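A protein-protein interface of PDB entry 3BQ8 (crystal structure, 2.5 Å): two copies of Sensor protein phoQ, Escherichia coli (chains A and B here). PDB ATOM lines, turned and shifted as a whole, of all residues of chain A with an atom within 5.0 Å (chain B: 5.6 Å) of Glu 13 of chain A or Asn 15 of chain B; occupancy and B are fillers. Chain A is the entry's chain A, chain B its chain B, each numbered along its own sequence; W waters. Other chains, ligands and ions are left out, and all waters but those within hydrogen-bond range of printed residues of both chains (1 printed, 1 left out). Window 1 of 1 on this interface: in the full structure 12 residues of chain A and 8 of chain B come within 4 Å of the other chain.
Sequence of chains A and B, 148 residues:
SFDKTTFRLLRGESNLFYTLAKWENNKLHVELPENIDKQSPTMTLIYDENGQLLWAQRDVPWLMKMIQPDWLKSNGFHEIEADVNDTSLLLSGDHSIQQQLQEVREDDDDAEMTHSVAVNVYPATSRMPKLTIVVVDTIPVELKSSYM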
ATOM      1  N   LEU A   9      29.315 -22.923 -28.892  1.00  0.00           N
ATOM      2  CA  LEU A   9      28.087 -23.404 -28.293  1.00  0.00           C
ATOM      3  C   LEU A   9      28.306 -24.738 -27.593  1.00  0.00           C
ATOM      4  O   LEU A   9      27.628 -25.056 -26.607  1.00  0.00           O
ATOM      5  CB  LEU A   9      26.987 -23.485 -29.363  1.00  0.00           C
ATOM      6  CG  LEU A   9      26.488 -24.796 -29.983  1.00  0.00           C
ATOM      7  CD1 LEU A   9      25.671 -25.596 -28.975  1.00  0.00           C
ATOM      8  CD2 LEU A   9      25.619 -24.441 -31.206  1.00  0.00           C
ATOM      9  N   LEU A  10      29.259 -25.512 -28.100  1.00  0.00           N
ATOM     10  CA  LEU A  10      29.596 -26.795 -27.505  1.00  0.00           C
ATOM     11  C   LEU A  10      30.418 -26.534 -26.232  1.00  0.00           C
ATOM     12  O   LEU A  10      30.222 -27.187 -25.205  1.00  0.00           O
ATOM     13  CB  LEU A  10      30.402 -27.649 -28.499  1.00  0.00           C
ATOM     14  CG  LEU A  10      29.647 -28.272 -29.686  1.00  0.00           C
ATOM     15  CD1 LEU A  10      30.535 -29.272 -30.402  1.00  0.00           C
ATOM     16  CD2 LEU A  10      28.406 -28.967 -29.196  1.00  0.00           C
ATOM     17  N   ARG A  11      31.344 -25.579 -26.294  1.00  0.00           N
ATOM     18  CA  ARG A  11      32.132 -25.273 -25.113  1.00  0.00           C
ATOM     19  C   ARG A  11      31.228 -24.667 -24.048  1.00  0.00           C
ATOM     20  O   ARG A  11      31.436 -24.868 -22.867  1.00  0.00           O
ATOM     21  CB  ARG A  11      33.285 -24.338 -25.457  1.00  0.00           C
ATOM     22  CG  ARG A  11      34.444 -25.035 -26.164  1.00  0.00           C
ATOM     23  CD  ARG A  11      35.627 -24.090 -26.357  1.00  0.00           C
ATOM     24  NE  ARG A  11      36.191 -23.587 -25.099  1.00  0.00           N
ATOM     25  CZ  ARG A  11      36.988 -24.283 -24.282  1.00  0.00           C
ATOM     26  NH1 ARG A  11      37.333 -25.536 -24.580  1.00  0.00           N
ATOM     27  NH2 ARG A  11      37.457 -23.712 -23.168  1.00  0.00           N
ATOM     28  N   GLY A  12      30.194 -23.958 -24.483  1.00  0.00           N
ATOM     29  CA  GLY A  12      29.247 -23.358 -23.558  1.00  0.00           C
ATOM     30  C   GLY A  12      28.361 -24.358 -22.833  1.00  0.00           C
ATOM     31  O   GLY A  12      27.976 -24.126 -21.678  1.00  0.00           O
ATOM     32  N   GLU A  13      28.011 -25.455 -23.506  1.00  0.00           N
ATOM     33  CA  GLU A  13      27.194 -26.510 -22.904  1.00  0.00           C
ATOM     34  C   GLU A  13      28.075 -27.275 -21.860  1.00  0.00           C
ATOM     35  O   GLU A  13      27.586 -27.769 -20.851  1.00  0.00           O
ATOM     36  CB  GLU A  13      26.686 -27.469 -23.993  1.00  0.00           C
ATOM     37  CG  GLU A  13      25.471 -28.312 -23.572  1.00  0.00           C
ATOM     38  CD  GLU A  13      24.184 -27.482 -23.435  1.00  0.00           C
ATOM     39  OE1 GLU A  13      23.284 -27.891 -22.669  1.00  0.00           O
ATOM     40  OE2 GLU A  13      24.062 -26.424 -24.102  1.00  0.00           O
ATOM     41  N   SER A  14      29.371 -27.372 -22.125  1.00  0.00           N
ATOM     42  CA  SER A  14      30.300 -28.019 -21.198  1.00  0.00           C
ATOM     43  C   SER A  14      30.232 -27.260 -19.845  1.00  0.00           C
ATOM     44  O   SER A  14      30.113 -27.860 -18.777  1.00  0.00           O
ATOM     45  CB  SER A  14      31.719 -27.970 -21.780  1.00  0.00           C
ATOM     46  OG  SER A  14      32.611 -28.796 -21.047  1.00  0.00           O
ATOM     47  N   ASN A  15      30.298 -25.937 -19.918  1.00  0.00           N
ATOM     48  CA  ASN A  15      30.209 -25.088 -18.740  1.00  0.00           C
ATOM     49  C   ASN A  15      28.900 -25.271 -18.005  1.00  0.00           C
ATOM     50  O   ASN A  15      28.878 -25.409 -16.795  1.00  0.00           O
ATOM     51  CB  ASN A  15      30.358 -23.640 -19.136  1.00  0.00           C
ATOM     52  CG  ASN A  15      31.790 -23.218 -19.211  1.00  0.00           C
ATOM     53  OD1 ASN A  15      32.683 -24.046 -19.377  1.00  0.00           O
ATOM     54  ND2 ASN A  15      32.027 -21.915 -19.094  1.00  0.00           N
ATOM     55  N   LEU A  16      27.788 -25.275 -18.721  1.00  0.00           N
ATOM     56  CA  LEU A  16      26.534 -25.458 -18.023  1.00  0.00           C
ATOM     57  C   LEU A  16      26.656 -26.692 -17.157  1.00  0.00           C
ATOM     58  O   LEU A  16      26.449 -26.621 -15.952  1.00  0.00           O
ATOM     59  CB  LEU A  16      25.363 -25.614 -18.993  1.00  0.00           C
ATOM     60  CG  LEU A  16      24.053 -25.795 -18.231  1.00  0.00           C
ATOM     61  CD1 LEU A  16      23.709 -24.475 -17.514  1.00  0.00           C
ATOM     62  CD2 LEU A  16      22.944 -26.234 -19.177  1.00  0.00           C
ATOM     63  N   PHE A  17      27.003 -27.824 -17.765  1.00  0.00           N
ATOM     64  CA  PHE A  17      27.151 -29.079 -17.021  1.00  0.00           C
ATOM     65  C   PHE A  17      28.197 -29.052 -15.894  1.00  0.00           C
ATOM     66  O   PHE A  17      28.018 -29.707 -14.878  1.00  0.00           O
ATOM     67  CB  PHE A  17      27.453 -30.228 -17.983  1.00  0.00           C
ATOM     68  CG  PHE A  17      26.238 -30.747 -18.692  1.00  0.00           C
ATOM     69  CD1 PHE A  17      25.576 -29.963 -19.632  1.00  0.00           C
ATOM     70  CD2 PHE A  17      25.735 -32.008 -18.399  1.00  0.00           C
ATOM     71  CE1 PHE A  17      24.426 -30.432 -20.266  1.00  0.00           C
ATOM     72  CE2 PHE A  17      24.588 -32.484 -19.030  1.00  0.00           C
ATOM     73  CZ  PHE A  17      23.934 -31.692 -19.964  1.00  0.00           C
ATOM     74  N   SER A  40      18.401 -29.384 -25.854  1.00  0.00           N
ATOM     75  CA  SER A  40      19.596 -29.182 -26.647  1.00  0.00           C
ATOM     76  C   SER A  40      19.936 -30.456 -27.381  1.00  0.00           C
ATOM     77  O   SER A  40      19.766 -31.540 -26.853  1.00  0.00           O
ATOM     78  CB  SER A  40      20.751 -28.776 -25.728  1.00  0.00           C
ATOM     79  OG  SER A  40      21.913 -28.434 -26.462  1.00  0.00           O
ATOM     80  N   THR A  42      22.584 -32.209 -28.018  1.00  0.00           N
ATOM     81  CA  THR A  42      23.939 -32.521 -27.573  1.00  0.00           C
ATOM     82  C   THR A  42      23.939 -33.764 -26.671  1.00  0.00           C
ATOM     83  O   THR A  42      22.912 -34.152 -26.129  1.00  0.00           O
ATOM     84  CB  THR A  42      24.531 -31.338 -26.749  1.00  0.00           C
ATOM     85  OG1 THR A  42      23.736 -31.105 -25.568  1.00  0.00           O
ATOM     86  CG2 THR A  42      24.533 -30.094 -27.556  1.00  0.00           C
ATOM     87  N   THR A  44      26.462 -35.402 -23.558  1.00  0.00           N
ATOM     88  CA  THR A  44      27.599 -35.120 -22.705  1.00  0.00           C
ATOM     89  C   THR A  44      28.114 -36.316 -21.911  1.00  0.00           C
ATOM     90  O   THR A  44      27.347 -37.156 -21.448  1.00  0.00           O
ATOM     91  CB  THR A  44      27.268 -33.971 -21.746  1.00  0.00           C
ATOM     92  OG1 THR A  44      26.869 -32.825 -22.515  1.00  0.00           O
ATOM     93  CG2 THR A  44      28.491 -33.619 -20.883  1.00  0.00           C
ATOM     94  N   VAL A 135      31.499 -33.005 -25.097  1.00  0.00           N
ATOM     95  CA  VAL A 135      30.204 -32.676 -25.643  1.00  0.00           C
ATOM     96  C   VAL A 135      30.129 -32.931 -27.144  1.00  0.00           C
ATOM     97  O   VAL A 135      30.925 -32.415 -27.938  1.00  0.00           O
ATOM     98  CB  VAL A 135      29.830 -31.211 -25.308  1.00  0.00           C
ATOM     99  CG1 VAL A 135      28.347 -30.950 -25.615  1.00  0.00           C
ATOM    100  CG2 VAL A 135      30.100 -30.960 -23.841  1.00  0.00           C
ATOM    101  N   LEU B  10      21.393 -18.322 -29.061  1.00  0.00           N
ATOM    102  CA  LEU B  10      20.908 -17.395 -28.068  1.00  0.00           C
ATOM    103  C   LEU B  10      20.948 -18.093 -26.713  1.00  0.00           C
ATOM    104  O   LEU B  10      21.321 -17.508 -25.722  1.00  0.00           O
ATOM    105  CB  LEU B  10      19.498 -16.940 -28.440  1.00  0.00           C
ATOM    106  CG  LEU B  10      19.425 -16.003 -29.667  1.00  0.00           C
ATOM    107  CD1 LEU B  10      17.973 -15.637 -29.902  1.00  0.00           C
ATOM    108  CD2 LEU B  10      20.270 -14.733 -29.476  1.00  0.00           C
ATOM    109  N   ARG B  11      20.583 -19.364 -26.696  1.00  0.00           N
ATOM    110  CA  ARG B  11      20.611 -20.168 -25.495  1.00  0.00           C
ATOM    111  C   ARG B  11      22.059 -20.441 -25.059  1.00  0.00           C
ATOM    112  O   ARG B  11      22.302 -20.888 -23.940  1.00  0.00           O
ATOM    113  CB  ARG B  11      19.877 -21.475 -25.750  1.00  0.00           C
ATOM    114  CG  ARG B  11      20.107 -22.550 -24.703  1.00  0.00           C
ATOM    115  CD  ARG B  11      19.201 -23.738 -24.969  1.00  0.00           C
ATOM    116  NE  ARG B  11      19.394 -24.821 -24.013  1.00  0.00           N
ATOM    117  CZ  ARG B  11      20.535 -25.479 -23.841  1.00  0.00           C
ATOM    118  NH1 ARG B  11      21.597 -25.155 -24.570  1.00  0.00           N
ATOM    119  NH2 ARG B  11      20.611 -26.457 -22.946  1.00  0.00           N
ATOM    120  N   GLY B  12      23.007 -20.184 -25.963  1.00  0.00           N
ATOM    121  CA  GLY B  12      24.405 -20.370 -25.653  1.00  0.00           C
ATOM    122  C   GLY B  12      24.897 -19.109 -24.966  1.00  0.00           C
ATOM    123  O   GLY B  12      25.799 -19.138 -24.150  1.00  0.00           O
ATOM    124  N   GLU B  13      24.299 -17.979 -25.310  1.00  0.00           N
ATOM    125  CA  GLU B  13      24.659 -16.710 -24.700  1.00  0.00           C
ATOM    126  C   GLU B  13      24.053 -16.691 -23.298  1.00  0.00           C
ATOM    127  O   GLU B  13      24.545 -16.002 -22.411  1.00  0.00           O
ATOM    128  CB  GLU B  13      24.082 -15.561 -25.515  1.00  0.00           C
ATOM    129  CG  GLU B  13      24.375 -14.186 -24.937  1.00  0.00           C
ATOM    130  CD  GLU B  13      25.846 -13.812 -25.031  1.00  0.00           C
ATOM    131  OE1 GLU B  13      26.240 -12.735 -24.528  1.00  0.00           O
ATOM    132  OE2 GLU B  13      26.614 -14.602 -25.619  1.00  0.00           O
ATOM    133  N   SER B  14      22.977 -17.461 -23.129  1.00  0.00           N
ATOM    134  CA  SER B  14      22.224 -17.583 -21.881  1.00  0.00           C
ATOM    135  C   SER B  14      22.961 -18.461 -20.859  1.00  0.00           C
ATOM    136  O   SER B  14      23.022 -18.132 -19.687  1.00  0.00           O
ATOM    137  CB  SER B  14      20.828 -18.176 -22.192  1.00  0.00           C
ATOM    138  OG  SER B  14      19.994 -18.275 -21.042  1.00  0.00           O
ATOM    139  N   ASN B  15      23.512 -19.580 -21.322  1.00  0.00           N
ATOM    140  CA  ASN B  15      24.233 -20.509 -20.460  1.00  0.00           C
ATOM    141  C   ASN B  15      25.521 -19.850 -19.978  1.00  0.00           C
ATOM    142  O   ASN B  15      26.043 -20.173 -18.899  1.00  0.00           O
ATOM    143  CB  ASN B  15      24.543 -21.800 -21.221  1.00  0.00           C
ATOM    144  CG  ASN B  15      23.325 -22.697 -21.370  1.00  0.00           C
ATOM    145  OD1 ASN B  15      23.305 -23.604 -22.196  1.00  0.00           O
ATOM    146  ND2 ASN B  15      22.309 -22.457 -20.561  1.00  0.00           N
ATOM    147  N   LEU B  16      26.010 -18.912 -20.788  1.00  0.00           N
ATOM    148  CA  LEU B  16      27.228 -18.174 -20.486  1.00  0.00           C
ATOM    149  C   LEU B  16      26.954 -17.317 -19.260  1.00  0.00           C
ATOM    150  O   LEU B  16      27.656 -17.395 -18.261  1.00  0.00           O
ATOM    151  CB  LEU B  16      27.592 -17.270 -21.667  1.00  0.00           C
ATOM    152  CG  LEU B  16      29.055 -16.991 -22.032  1.00  0.00           C
ATOM    153  CD1 LEU B  16      29.623 -18.178 -22.804  1.00  0.00           C
ATOM    154  CD2 LEU B  16      29.132 -15.741 -22.903  1.00  0.00           C
ATOM    155  N   PHE B  17      25.920 -16.496 -19.357  1.00  0.00           N
ATOM    156  CA  PHE B  17      25.513 -15.607 -18.284  1.00  0.00           C
ATOM    157  C   PHE B  17      25.148 -16.309 -16.991  1.00  0.00           C
ATOM    158  O   PHE B  17      25.232 -15.717 -15.911  1.00  0.00           O
ATOM    159  CB  PHE B  17      24.325 -14.796 -18.737  1.00  0.00           C
ATOM    160  CG  PHE B  17      24.693 -13.500 -19.362  1.00  0.00           C
ATOM    161  CD1 PHE B  17      24.909 -12.377 -18.572  1.00  0.00           C
ATOM    162  CD2 PHE B  17      24.775 -13.381 -20.746  1.00  0.00           C
ATOM    163  CE1 PHE B  17      25.189 -11.155 -19.151  1.00  0.00           C
ATOM    164  CE2 PHE B  17      25.054 -12.159 -21.330  1.00  0.00           C
ATOM    165  CZ  PHE B  17      25.260 -11.045 -20.535  1.00  0.00           C
ATOM    166  N   TYR B  18      24.711 -17.558 -17.118  1.00  0.00           N
ATOM    167  CA  TYR B  18      24.328 -18.371 -15.980  1.00  0.00           C
ATOM    168  C   TYR B  18      25.567 -18.948 -15.310  1.00  0.00           C
ATOM    169  O   TYR B  18      25.577 -19.192 -14.107  1.00  0.00           O
ATOM    170  CB  TYR B  18      23.429 -19.517 -16.434  1.00  0.00           C
ATOM    171  CG  TYR B  18      22.973 -20.390 -15.299  1.00  0.00           C
ATOM    172  CD1 TYR B  18      21.962 -19.973 -14.455  1.00  0.00           C
ATOM    173  CD2 TYR B  18      23.601 -21.602 -15.021  1.00  0.00           C
ATOM    174  CE1 TYR B  18      21.585 -20.719 -13.359  1.00  0.00           C
ATOM    175  CE2 TYR B  18      23.224 -22.367 -13.917  1.00  0.00           C
ATOM    176  CZ  TYR B  18      22.215 -21.909 -13.086  1.00  0.00           C
ATOM    177  OH  TYR B  18      21.853 -22.602 -11.948  1.00  0.00           O
ATOM    178  N   THR B  19      26.614 -19.171 -16.095  1.00  0.00           N
ATOM    179  CA  THR B  19      27.839 -19.733 -15.560  1.00  0.00           C
ATOM    180  C   THR B  19      28.668 -18.681 -14.860  1.00  0.00           C
ATOM    181  O   THR B  19      29.412 -18.986 -13.940  1.00  0.00           O
ATOM    182  CB  THR B  19      28.705 -20.419 -16.660  1.00  0.00           C
ATOM    183  OG1 THR B  19      28.884 -19.526 -17.765  1.00  0.00           O
ATOM    184  CG2 THR B  19      28.050 -21.707 -17.134  1.00  0.00           C
ATOM    185  N   LEU B  20      28.532 -17.441 -15.287  1.00  0.00           N
ATOM    186  CA  LEU B  20      29.286 -16.352 -14.690  1.00  0.00           C
ATOM    187  C   LEU B  20      28.551 -15.754 -13.495  1.00  0.00           C
ATOM    188  O   LEU B  20      29.149 -15.077 -12.665  1.00  0.00           O
ATOM    189  CB  LEU B  20      29.551 -15.273 -15.744  1.00  0.00           C
ATOM    190  CG  LEU B  20      30.409 -15.764 -16.921  1.00  0.00           C
ATOM    191  CD1 LEU B  20      30.648 -14.639 -17.915  1.00  0.00           C
ATOM    192  CD2 LEU B  20      31.736 -16.305 -16.380  1.00  0.00           C
ATOM    193  N   TYR B 122      16.226 -21.916 -15.508  1.00  0.00           N
ATOM    194  CA  TYR B 122      17.215 -22.657 -14.758  1.00  0.00           C
ATOM    195  C   TYR B 122      16.669 -22.894 -13.366  1.00  0.00           C
ATOM    196  O   TYR B 122      16.601 -21.979 -12.537  1.00  0.00           O
ATOM    197  CB  TYR B 122      18.522 -21.883 -14.700  1.00  0.00           C
ATOM    198  CG  TYR B 122      19.081 -21.526 -16.066  1.00  0.00           C
ATOM    199  CD1 TYR B 122      18.624 -20.414 -16.758  1.00  0.00           C
ATOM    200  CD2 TYR B 122      20.084 -22.295 -16.654  1.00  0.00           C
ATOM    201  CE1 TYR B 122      19.152 -20.071 -17.993  1.00  0.00           C
ATOM    202  CE2 TYR B 122      20.621 -21.962 -17.887  1.00  0.00           C
ATOM    203  CZ  TYR B 122      20.154 -20.853 -18.551  1.00  0.00           C
ATOM    204  OH  TYR B 122      20.687 -20.524 -19.775  1.00  0.00           O
ATOM    205  N   ILE B 133      16.559 -16.712 -17.771  1.00  0.00           N
ATOM    206  CA  ILE B 133      17.385 -15.764 -18.490  1.00  0.00           C
ATOM    207  C   ILE B 133      16.722 -15.574 -19.851  1.00  0.00           C
ATOM    208  O   ILE B 133      16.244 -16.526 -20.478  1.00  0.00           O
ATOM    209  CB  ILE B 133      18.818 -16.277 -18.646  1.00  0.00           C
ATOM    210  CG1 ILE B 133      19.401 -16.568 -17.260  1.00  0.00           C
ATOM    211  CG2 ILE B 133      19.667 -15.244 -19.418  1.00  0.00           C
ATOM    212  CD1 ILE B 133      20.836 -16.984 -17.293  1.00  0.00           C
HETATM  213  O   HOH W   1      29.885 -20.300 -20.871  1.00  0.00           O
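Among the printed residues, merely in contact across the chains: Asn 15 of chain A with Thr 19 of chain B (3.6 Å), Ser 40 of chain A with Arg 11 of chain B (3.6 Å), Leu 16 of chain A with Tyr 18 of chain B (3.8 Å), Leu 16 of chain A with Asn 15 of chain B (3.9 Å), Leu 16 of chain A with Thr 19 of chain B (3.9 Å) and Leu 16 of chain A with Tyr 122 of chain B (3.999 Å).
The side-chain carboxylate of Glu 13 of chain A lies within salt-bridge range of the guanidinium group of Arg 11 of chain B (2.8 Å). OE2 of Glu 13 of chain A lies close to OD1 of Asn 15 of chain B (3.5 Å).
The side-chain hydroxyl (OH) of Tyr 122 of chain B lies within hydrogen-bond range of the side-chain amide nitrogen (ND2) of Asn 15 of chain B. The side-chain hydroxyl of Ser 40 of chain A lies close to the side-chain hydroxyl of Thr 42 of chain A (3.4 Å). OG of Ser 14 of chain B sits at hydrogen-bond distance from OH of Tyr 122 of chain B (2.7 Å). The side-chain hydroxyl of Thr 19 of chain B is in hydrogen-bond range of the backbone carbonyl oxygen of Leu 16 of chain B (2.5 Å). OD1 of Asn 15 of chain B sits at hydrogen-bond distance from NH1 of Arg 11 of chain B (3.3 Å). OG1 of Thr 19 of chain B lies close to O of Asn 15 of chain B, 3.1 Å away.
Glu 13 of chain A touches Arg 11 of chain B, but with the chains exchanged Arg 11 of chain A does not touch Glu 13 of chain B (9.7 Å). Glu 13 of chain A touches Asn 15 of chain B, but with the chains exchanged Asn 15 of chain A does not touch Glu 13 of chain B (10.1 Å). Leu 16 of chain A touches Asn 15 of chain B, but with the chains exchanged Asn 15 of chain A does not touch Leu 16 of chain B (5.8 Å). Positions printed for both chains: 10, 11, 12, 13, 14, 15, 16 and 17. Of the 8 pairs that touch across the chains among the printed residues, none has its exchanged pair printed and touching as well.
Water W1 lies within hydrogen-bond range of ND2 of Asn 15 of chain A and OG1 of Thr 19 of chain B.
Of chain B, only Arg 11 (2.8 Å) and Asn 15 (3.5 Å) come within 4 Å of Glu 13 of chain A. Of chain A, only Glu 13 (3.5 Å) and Leu 16 (3.9 Å) come within 4 Å of Asn 15 of chain B. Of the printed residues of chain A, Tyr 18 of chain B touches Leu 16 (3.8 Å). Of the printed residues of chain B, Asn 15 of chain A touches Thr 19 (3.6 Å). Thr 42 of chain A touches none of the printed residues of chain B. Leu 20 of chain B touches none of the printed residues of chain A. The nearest residue of chain A that does not touch Asn 15 of chain B is Gly 12 of chain A (4.2 Å). The nearest printed residue of chain A that does not touch Tyr 122 of chain B is Glu 13 of chain A (8.1 Å).
Hydrophobic or aromatic side chains of chain A within 4 Å of the printed part of chain B: Leu 16. Hydrophobic or aromatic side chains of chain B within 4 Å of the printed part of chain A: Tyr 18 and Tyr 122. Along chain B the printed residues that touch a printed residue of chain A span positions 11 to 122. Among the printed residues, Asp or Glu carboxylates within 4 Å of a Lys or Arg side-chain nitrogen of the other chain: Glu 13 of chain A with Arg 11 of chain B (2.8 Å).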
